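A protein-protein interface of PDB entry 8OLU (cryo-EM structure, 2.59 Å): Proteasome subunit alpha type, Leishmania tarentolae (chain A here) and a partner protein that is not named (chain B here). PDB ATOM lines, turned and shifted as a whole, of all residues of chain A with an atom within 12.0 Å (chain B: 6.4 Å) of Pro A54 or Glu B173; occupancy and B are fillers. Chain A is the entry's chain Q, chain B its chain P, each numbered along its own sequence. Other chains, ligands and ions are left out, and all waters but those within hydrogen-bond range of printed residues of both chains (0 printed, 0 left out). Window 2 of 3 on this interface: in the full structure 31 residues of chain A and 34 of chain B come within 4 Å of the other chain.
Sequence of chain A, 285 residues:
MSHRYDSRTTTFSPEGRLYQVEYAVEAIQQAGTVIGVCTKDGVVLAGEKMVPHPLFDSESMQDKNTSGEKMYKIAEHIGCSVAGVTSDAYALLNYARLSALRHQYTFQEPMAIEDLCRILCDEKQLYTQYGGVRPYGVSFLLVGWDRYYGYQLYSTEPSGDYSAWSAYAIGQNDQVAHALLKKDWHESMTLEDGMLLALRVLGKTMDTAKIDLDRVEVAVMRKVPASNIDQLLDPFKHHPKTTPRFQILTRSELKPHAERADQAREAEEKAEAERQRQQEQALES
N of Lys B157 is in hydrogen-bond range of O of Leu A55 (2.7 Å).
NZ of Lys B157 sits at hydrogen-bond distance from O of Phe A56, 3.0 Å away.
ND1 of His A53 sits close to N of Leu A55, at 3.3 Å.
Glu B173 touches His A53.
Pro A54 touches Lys B157.
Glu B173 touches Pro A54.
Leu A55 touches Ala B158.
Leu A55 touches Tyr B176.
Asp A57 touches Lys B157 (CB to CG, 3.9 Å).
Printed residues of chain B within 4 Å of His A53: Glu B173 (3.6 Å).
Pro A54 touches just these residues of chain B: Lys B157 (3.7 Å) and Glu B173 (3.0 Å).
Printed residues of chain B within 4 Å of Phe A56: Lys B157 (3.0 Å).
Ala B158 touches just one residue of chain A: Leu A55 (3.6 Å).
No residue of chain A comes within 4 Å of Ala B170.
Leu B172 touches none of the printed residues of chain A.
Lys B174 touches none of the printed residues of chain A.
The nearest printed residue of chain B that does not touch Asp A57 is Tyr B176 (6.2 Å).
Hydrophobic or aromatic side chains of chain B that line the printed part of chain A: Tyr B176.
Of the 15 printed residues of chain A, 5 touch a printed residue of chain B.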
ATOM      1  N   LYS A  49      24.016  11.621  18.308  1.00  0.00           N
ATOM      2  CA  LYS A  49      23.678  12.275  17.051  1.00  0.00           C
ATOM      3  C   LYS A  49      24.870  12.254  16.094  1.00  0.00           C
ATOM      4  O   LYS A  49      26.005  12.057  16.514  1.00  0.00           O
ATOM      5  CB  LYS A  49      23.363  13.739  17.342  1.00  0.00           C
ATOM      6  CG  LYS A  49      22.403  13.944  18.493  1.00  0.00           C
ATOM      7  CD  LYS A  49      21.541  15.153  18.394  1.00  0.00           C
ATOM      8  CE  LYS A  49      22.266  16.441  18.694  1.00  0.00           C
ATOM      9  NZ  LYS A  49      21.291  17.497  19.045  1.00  0.00           N
ATOM     10  N   MET A  50      24.650  12.516  14.808  1.00  0.00           N
ATOM     11  CA  MET A  50      25.788  12.656  13.910  1.00  0.00           C
ATOM     12  C   MET A  50      26.340  14.068  14.086  1.00  0.00           C
ATOM     13  O   MET A  50      25.690  14.909  14.706  1.00  0.00           O
ATOM     14  CB  MET A  50      25.453  12.365  12.440  1.00  0.00           C
ATOM     15  CG  MET A  50      24.522  13.369  11.757  1.00  0.00           C
ATOM     16  SD  MET A  50      24.610  13.291   9.910  1.00  0.00           S
ATOM     17  CE  MET A  50      26.323  13.713   9.554  1.00  0.00           C
ATOM     18  N   VAL A  51      27.546  14.292  13.546  1.00  0.00           N
ATOM     19  CA  VAL A  51      28.327  15.497  13.800  1.00  0.00           C
ATOM     20  C   VAL A  51      27.587  16.691  13.203  1.00  0.00           C
ATOM     21  O   VAL A  51      27.237  16.678  12.022  1.00  0.00           O
ATOM     22  CB  VAL A  51      29.754  15.416  13.210  1.00  0.00           C
ATOM     23  CG1 VAL A  51      30.677  16.444  13.865  1.00  0.00           C
ATOM     24  CG2 VAL A  51      30.342  14.005  13.274  1.00  0.00           C
ATOM     25  N   PRO A  52      27.355  17.763  13.984  1.00  0.00           N
ATOM     26  CA  PRO A  52      26.468  18.843  13.559  1.00  0.00           C
ATOM     27  C   PRO A  52      27.186  19.908  12.729  1.00  0.00           C
ATOM     28  O   PRO A  52      27.677  20.897  13.268  1.00  0.00           O
ATOM     29  CB  PRO A  52      25.971  19.382  14.904  1.00  0.00           C
ATOM     30  CG  PRO A  52      27.191  19.231  15.803  1.00  0.00           C
ATOM     31  CD  PRO A  52      27.964  18.025  15.292  1.00  0.00           C
ATOM     32  N   HIS A  53      27.261  19.652  11.413  1.00  0.00           N
ATOM     33  CA  HIS A  53      27.525  20.650  10.386  1.00  0.00           C
ATOM     34  C   HIS A  53      26.876  21.967  10.803  1.00  0.00           C
ATOM     35  O   HIS A  53      25.725  21.975  11.227  1.00  0.00           O
ATOM     36  CB  HIS A  53      26.964  20.129   9.055  1.00  0.00           C
ATOM     37  CG  HIS A  53      27.455  20.785   7.796  1.00  0.00           C
ATOM     38  ND1 HIS A  53      27.347  22.136   7.526  1.00  0.00           N
ATOM     39  CD2 HIS A  53      27.995  20.187   6.687  1.00  0.00           C
ATOM     40  CE1 HIS A  53      27.835  22.368   6.306  1.00  0.00           C
ATOM     41  NE2 HIS A  53      28.244  21.167   5.763  1.00  0.00           N
ATOM     42  N   PRO A  54      27.569  23.121  10.693  1.00  0.00           N
ATOM     43  CA  PRO A  54      27.014  24.399  11.177  1.00  0.00           C
ATOM     44  C   PRO A  54      25.885  25.008  10.339  1.00  0.00           C
ATOM     45  O   PRO A  54      25.379  26.088  10.635  1.00  0.00           O
ATOM     46  CB  PRO A  54      28.213  25.345  11.104  1.00  0.00           C
ATOM     47  CG  PRO A  54      29.038  24.755   9.950  1.00  0.00           C
ATOM     48  CD  PRO A  54      28.888  23.249  10.050  1.00  0.00           C
ATOM     49  N   LEU A  55      25.495  24.288   9.285  1.00  0.00           N
ATOM     50  CA  LEU A  55      24.446  24.713   8.383  1.00  0.00           C
ATOM     51  C   LEU A  55      23.173  23.914   8.568  1.00  0.00           C
ATOM     52  O   LEU A  55      22.228  24.176   7.845  1.00  0.00           O
ATOM     53  CB  LEU A  55      24.945  24.542   6.956  1.00  0.00           C
ATOM     54  CG  LEU A  55      25.792  25.694   6.413  1.00  0.00           C
ATOM     55  CD1 LEU A  55      26.131  25.439   4.952  1.00  0.00           C
ATOM     56  CD2 LEU A  55      25.085  27.032   6.582  1.00  0.00           C
ATOM     57  N   PHE A  56      23.141  22.980   9.527  1.00  0.00           N
ATOM     58  CA  PHE A  56      21.922  22.266   9.848  1.00  0.00           C
ATOM     59  C   PHE A  56      20.948  23.232  10.466  1.00  0.00           C
ATOM     60  O   PHE A  56      21.351  24.089  11.227  1.00  0.00           O
ATOM     61  CB  PHE A  56      22.157  21.178  10.881  1.00  0.00           C
ATOM     62  CG  PHE A  56      22.832  19.938  10.362  1.00  0.00           C
ATOM     63  CD1 PHE A  56      22.905  19.656   9.002  1.00  0.00           C
ATOM     64  CD2 PHE A  56      23.400  19.028  11.245  1.00  0.00           C
ATOM     65  CE1 PHE A  56      23.530  18.498   8.537  1.00  0.00           C
ATOM     66  CE2 PHE A  56      24.037  17.877  10.775  1.00  0.00           C
ATOM     67  CZ  PHE A  56      24.104  17.608   9.420  1.00  0.00           C
ATOM     68  N   ASP A  57      19.674  23.083  10.151  1.00  0.00           N
ATOM     69  CA  ASP A  57      18.651  23.874  10.793  1.00  0.00           C
ATOM     70  C   ASP A  57      17.831  22.950  11.685  1.00  0.00           C
ATOM     71  O   ASP A  57      18.026  21.736  11.713  1.00  0.00           O
ATOM     72  CB  ASP A  57      17.798  24.588   9.755  1.00  0.00           C
ATOM     73  CG  ASP A  57      17.006  25.780  10.290  1.00  0.00           C
ATOM     74  OD1 ASP A  57      17.076  26.045  11.529  1.00  0.00           O
ATOM     75  OD2 ASP A  57      16.322  26.465   9.467  1.00  0.00           O
ATOM     76  N   SER A  58      17.011  23.558  12.529  1.00  0.00           N
ATOM     77  CA  SER A  58      15.999  22.811  13.224  1.00  0.00           C
ATOM     78  C   SER A  58      14.796  22.790  12.302  1.00  0.00           C
ATOM     79  O   SER A  58      14.610  23.708  11.517  1.00  0.00           O
ATOM     80  CB  SER A  58      15.662  23.426  14.568  1.00  0.00           C
ATOM     81  OG  SER A  58      14.658  24.436  14.448  1.00  0.00           O
ATOM     82  N   GLU A  69      16.472  13.616  16.807  1.00  0.00           N
ATOM     83  CA  GLU A  69      17.271  13.051  15.759  1.00  0.00           C
ATOM     84  C   GLU A  69      17.345  11.536  15.983  1.00  0.00           C
ATOM     85  O   GLU A  69      17.300  10.726  15.049  1.00  0.00           O
ATOM     86  CB  GLU A  69      18.579  13.840  15.807  1.00  0.00           C
ATOM     87  CG  GLU A  69      19.445  13.692  14.562  1.00  0.00           C
ATOM     88  CD  GLU A  69      20.818  14.338  14.692  1.00  0.00           C
ATOM     89  OE1 GLU A  69      21.824  13.584  14.577  1.00  0.00           O
ATOM     90  OE2 GLU A  69      20.870  15.594  14.921  1.00  0.00           O
ATOM     91  N   ASP A 212      29.891  15.726  24.616  1.00  0.00           N
ATOM     92  CA  ASP A 212      29.800  16.755  23.587  1.00  0.00           C
ATOM     93  C   ASP A 212      28.335  17.129  23.325  1.00  0.00           C
ATOM     94  O   ASP A 212      27.717  16.613  22.403  1.00  0.00           O
ATOM     95  CB  ASP A 212      30.488  16.268  22.303  1.00  0.00           C
ATOM     96  CG  ASP A 212      30.585  17.327  21.210  1.00  0.00           C
ATOM     97  OD1 ASP A 212      30.239  18.521  21.493  1.00  0.00           O
ATOM     98  OD2 ASP A 212      30.991  16.954  20.077  1.00  0.00           O
ATOM     99  N   ASP A 214      26.571  18.804  21.745  1.00  0.00           N
ATOM    100  CA  ASP A 214      26.183  18.915  20.352  1.00  0.00           C
ATOM    101  C   ASP A 214      25.875  17.544  19.745  1.00  0.00           C
ATOM    102  O   ASP A 214      25.003  17.468  18.891  1.00  0.00           O
ATOM    103  CB  ASP A 214      27.318  19.541  19.527  1.00  0.00           C
ATOM    104  CG  ASP A 214      27.356  21.062  19.454  1.00  0.00           C
ATOM    105  OD1 ASP A 214      27.601  21.592  18.341  1.00  0.00           O
ATOM    106  OD2 ASP A 214      27.144  21.702  20.500  1.00  0.00           O
ATOM    107  N   ARG A 215      26.620  16.495  20.143  1.00  0.00           N
ATOM    108  CA  ARG A 215      26.520  15.153  19.577  1.00  0.00           C
ATOM    109  C   ARG A 215      25.644  14.207  20.417  1.00  0.00           C
ATOM    110  O   ARG A 215      25.642  12.992  20.177  1.00  0.00           O
ATOM    111  CB  ARG A 215      27.908  14.504  19.450  1.00  0.00           C
ATOM    112  CG  ARG A 215      28.655  14.866  18.173  1.00  0.00           C
ATOM    113  CD  ARG A 215      30.125  14.481  18.162  1.00  0.00           C
ATOM    114  NE  ARG A 215      30.360  13.088  17.783  1.00  0.00           N
ATOM    115  CZ  ARG A 215      31.333  12.320  18.274  1.00  0.00           C
ATOM    116  NH1 ARG A 215      31.283  11.003  18.124  1.00  0.00           N
ATOM    117  NH2 ARG A 215      32.327  12.869  18.953  1.00  0.00           N
ATOM    118  N   ARG A 251      19.077  21.090  25.107  1.00  0.00           N
ATOM    119  CA  ARG A 251      20.488  21.255  25.407  1.00  0.00           C
ATOM    120  C   ARG A 251      20.675  21.808  26.825  1.00  0.00           C
ATOM    121  O   ARG A 251      21.605  21.411  27.518  1.00  0.00           O
ATOM    122  CB  ARG A 251      21.084  22.174  24.339  1.00  0.00           C
ATOM    123  CG  ARG A 251      22.597  22.285  24.381  1.00  0.00           C
ATOM    124  CD  ARG A 251      23.039  23.658  23.908  1.00  0.00           C
ATOM    125  NE  ARG A 251      24.478  23.672  23.683  1.00  0.00           N
ATOM    126  CZ  ARG A 251      25.102  22.914  22.787  1.00  0.00           C
ATOM    127  NH1 ARG A 251      24.476  22.539  21.680  1.00  0.00           N
ATOM    128  NH2 ARG A 251      26.351  22.540  23.004  1.00  0.00           N
ATOM    129  N   LYS B 157      20.093  25.176   6.580  1.00  0.00           N
ATOM    130  CA  LYS B 157      19.984  26.618   6.469  1.00  0.00           C
ATOM    131  C   LYS B 157      20.474  27.021   5.099  1.00  0.00           C
ATOM    132  O   LYS B 157      20.140  28.075   4.572  1.00  0.00           O
ATOM    133  CB  LYS B 157      20.881  27.302   7.478  1.00  0.00           C
ATOM    134  CG  LYS B 157      20.324  27.369   8.882  1.00  0.00           C
ATOM    135  CD  LYS B 157      21.492  27.427   9.843  1.00  0.00           C
ATOM    136  CE  LYS B 157      21.093  27.609  11.288  1.00  0.00           C
ATOM    137  NZ  LYS B 157      22.075  26.884  12.131  1.00  0.00           N
ATOM    138  N   ALA B 158      21.278  26.148   4.536  1.00  0.00           N
ATOM    139  CA  ALA B 158      21.744  26.373   3.203  1.00  0.00           C
ATOM    140  C   ALA B 158      22.359  25.094   2.729  1.00  0.00           C
ATOM    141  O   ALA B 158      23.042  24.434   3.489  1.00  0.00           O
ATOM    142  CB  ALA B 158      22.789  27.433   3.236  1.00  0.00           C
ATOM    143  N   ALA B 168      30.388  24.297  -3.680  1.00  0.00           N
ATOM    144  CA  ALA B 168      29.225  25.126  -3.412  1.00  0.00           C
ATOM    145  C   ALA B 168      28.799  25.102  -1.949  1.00  0.00           C
ATOM    146  O   ALA B 168      28.348  26.133  -1.461  1.00  0.00           O
ATOM    147  CB  ALA B 168      28.056  24.687  -4.257  1.00  0.00           C
ATOM    148  N   LYS B 169      28.862  23.952  -1.273  1.00  0.00           N
ATOM    149  CA  LYS B 169      28.533  23.924   0.148  1.00  0.00           C
ATOM    150  C   LYS B 169      29.585  24.686   0.955  1.00  0.00           C
ATOM    151  O   LYS B 169      29.218  25.409   1.893  1.00  0.00           O
ATOM    152  CB  LYS B 169      28.375  22.505   0.720  1.00  0.00           C
ATOM    153  CG  LYS B 169      26.937  22.111   1.053  1.00  0.00           C
ATOM    154  CD  LYS B 169      26.777  20.726   1.614  1.00  0.00           C
ATOM    155  CE  LYS B 169      27.186  19.666   0.613  1.00  0.00           C
ATOM    156  NZ  LYS B 169      27.289  18.337   1.258  1.00  0.00           N
ATOM    157  N   ALA B 170      30.871  24.483   0.585  1.00  0.00           N
ATOM    158  CA  ALA B 170      31.997  25.120   1.261  1.00  0.00           C
ATOM    159  C   ALA B 170      31.870  26.639   1.171  1.00  0.00           C
ATOM    160  O   ALA B 170      32.144  27.334   2.143  1.00  0.00           O
ATOM    161  CB  ALA B 170      33.311  24.660   0.678  1.00  0.00           C
ATOM    162  N   PHE B 171      31.425  27.124   0.004  1.00  0.00           N
ATOM    163  CA  PHE B 171      31.327  28.542  -0.278  1.00  0.00           C
ATOM    164  C   PHE B 171      30.069  29.121   0.367  1.00  0.00           C
ATOM    165  O   PHE B 171      29.990  30.316   0.610  1.00  0.00           O
ATOM    166  CB  PHE B 171      31.445  28.760  -1.793  1.00  0.00           C
ATOM    167  CG  PHE B 171      31.171  30.157  -2.307  1.00  0.00           C
ATOM    168  CD1 PHE B 171      32.203  30.950  -2.784  1.00  0.00           C
ATOM    169  CD2 PHE B 171      29.878  30.666  -2.364  1.00  0.00           C
ATOM    170  CE1 PHE B 171      31.950  32.223  -3.278  1.00  0.00           C
ATOM    171  CE2 PHE B 171      29.627  31.928  -2.879  1.00  0.00           C
ATOM    172  CZ  PHE B 171      30.660  32.704  -3.336  1.00  0.00           C
ATOM    173  N   LEU B 172      29.084  28.291   0.677  1.00  0.00           N
ATOM    174  CA  LEU B 172      27.900  28.766   1.376  1.00  0.00           C
ATOM    175  C   LEU B 172      28.161  28.847   2.868  1.00  0.00           C
ATOM    176  O   LEU B 172      27.488  29.605   3.557  1.00  0.00           O
ATOM    177  CB  LEU B 172      26.743  27.807   1.110  1.00  0.00           C
ATOM    178  CG  LEU B 172      25.898  28.128  -0.114  1.00  0.00           C
ATOM    179  CD1 LEU B 172      24.924  26.980  -0.390  1.00  0.00           C
ATOM    180  CD2 LEU B 172      25.163  29.457   0.080  1.00  0.00           C
ATOM    181  N   GLU B 173      29.092  28.025   3.361  1.00  0.00           N
ATOM    182  CA  GLU B 173      29.455  28.020   4.767  1.00  0.00           C
ATOM    183  C   GLU B 173      30.042  29.386   5.147  1.00  0.00           C
ATOM    184  O   GLU B 173      29.581  29.997   6.116  1.00  0.00           O
ATOM    185  CB  GLU B 173      30.391  26.840   5.017  1.00  0.00           C
ATOM    186  CG  GLU B 173      30.684  26.571   6.485  1.00  0.00           C
ATOM    187  CD  GLU B 173      30.967  25.106   6.791  1.00  0.00           C
ATOM    188  OE1 GLU B 173      31.262  24.794   7.961  1.00  0.00           O
ATOM    189  OE2 GLU B 173      30.876  24.272   5.856  1.00  0.00           O
ATOM    190  N   LYS B 174      31.001  29.881   4.338  1.00  0.00           N
ATOM    191  CA  LYS B 174      31.553  31.220   4.500  1.00  0.00           C
ATOM    192  C   LYS B 174      30.459  32.290   4.512  1.00  0.00           C
ATOM    193  O   LYS B 174      30.290  32.994   5.501  1.00  0.00           O
ATOM    194  CB  LYS B 174      32.502  31.608   3.362  1.00  0.00           C
ATOM    195  CG  LYS B 174      33.782  30.800   3.248  1.00  0.00           C
ATOM    196  CD  LYS B 174      34.720  31.363   2.174  1.00  0.00           C
ATOM    197  CE  LYS B 174      35.128  30.369   1.096  1.00  0.00           C
ATOM    198  NZ  LYS B 174      35.524  29.048   1.648  1.00  0.00           N
ATOM    199  N   ARG B 175      29.720  32.401   3.405  1.00  0.00           N
ATOM    200  CA  ARG B 175      28.921  33.583   3.116  1.00  0.00           C
ATOM    201  C   ARG B 175      27.589  33.568   3.868  1.00  0.00           C
ATOM    202  O   ARG B 175      26.848  34.546   3.842  1.00  0.00           O
ATOM    203  CB  ARG B 175      28.670  33.735   1.604  1.00  0.00           C
ATOM    204  CG  ARG B 175      29.930  33.816   0.738  1.00  0.00           C
ATOM    205  CD  ARG B 175      29.911  34.927  -0.311  1.00  0.00           C
ATOM    206  NE  ARG B 175      28.555  35.367  -0.660  1.00  0.00           N
ATOM    207  CZ  ARG B 175      28.138  36.637  -0.692  1.00  0.00           C
ATOM    208  NH1 ARG B 175      26.844  36.927  -0.714  1.00  0.00           N
ATOM    209  NH2 ARG B 175      29.025  37.615  -0.720  1.00  0.00           N
ATOM    210  N   TYR B 176      27.260  32.471   4.536  1.00  0.00           N
ATOM    211  CA  TYR B 176      25.962  32.391   5.170  1.00  0.00           C
ATOM    212  C   TYR B 176      26.030  33.037   6.544  1.00  0.00           C
ATOM    213  O   TYR B 176      26.981  32.830   7.290  1.00  0.00           O
ATOM    214  CB  TYR B 176      25.494  30.936   5.292  1.00  0.00           C
ATOM    215  CG  TYR B 176      24.110  30.842   5.871  1.00  0.00           C
ATOM    216  CD1 TYR B 176      23.014  31.121   5.075  1.00  0.00           C
ATOM    217  CD2 TYR B 176      23.892  30.636   7.228  1.00  0.00           C
ATOM    218  CE1 TYR B 176      21.727  31.117   5.595  1.00  0.00           C
ATOM    219  CE2 TYR B 176      22.606  30.661   7.762  1.00  0.00           C
ATOM    220  CZ  TYR B 176      21.509  30.885   6.938  1.00  0.00           C
ATOM    221  OH  TYR B 176      20.199  30.894   7.392  1.00  0.00           O
ATOM    222  N   THR B 177      24.981  33.783   6.878  1.00  0.00           N
ATOM    223  CA  THR B 177      24.847  34.457   8.162  1.00  0.00           C
ATOM    224  C   THR B 177      23.397  34.288   8.621  1.00  0.00           C
ATOM    225  O   THR B 177      22.468  34.320   7.821  1.00  0.00           O
ATOM    226  CB  THR B 177      25.335  35.917   8.042  1.00  0.00           C
ATOM    227  OG1 THR B 177      24.889  36.494   6.808  1.00  0.00           O
ATOM    228  CG2 THR B 177      26.847  36.029   8.081  1.00  0.00           C
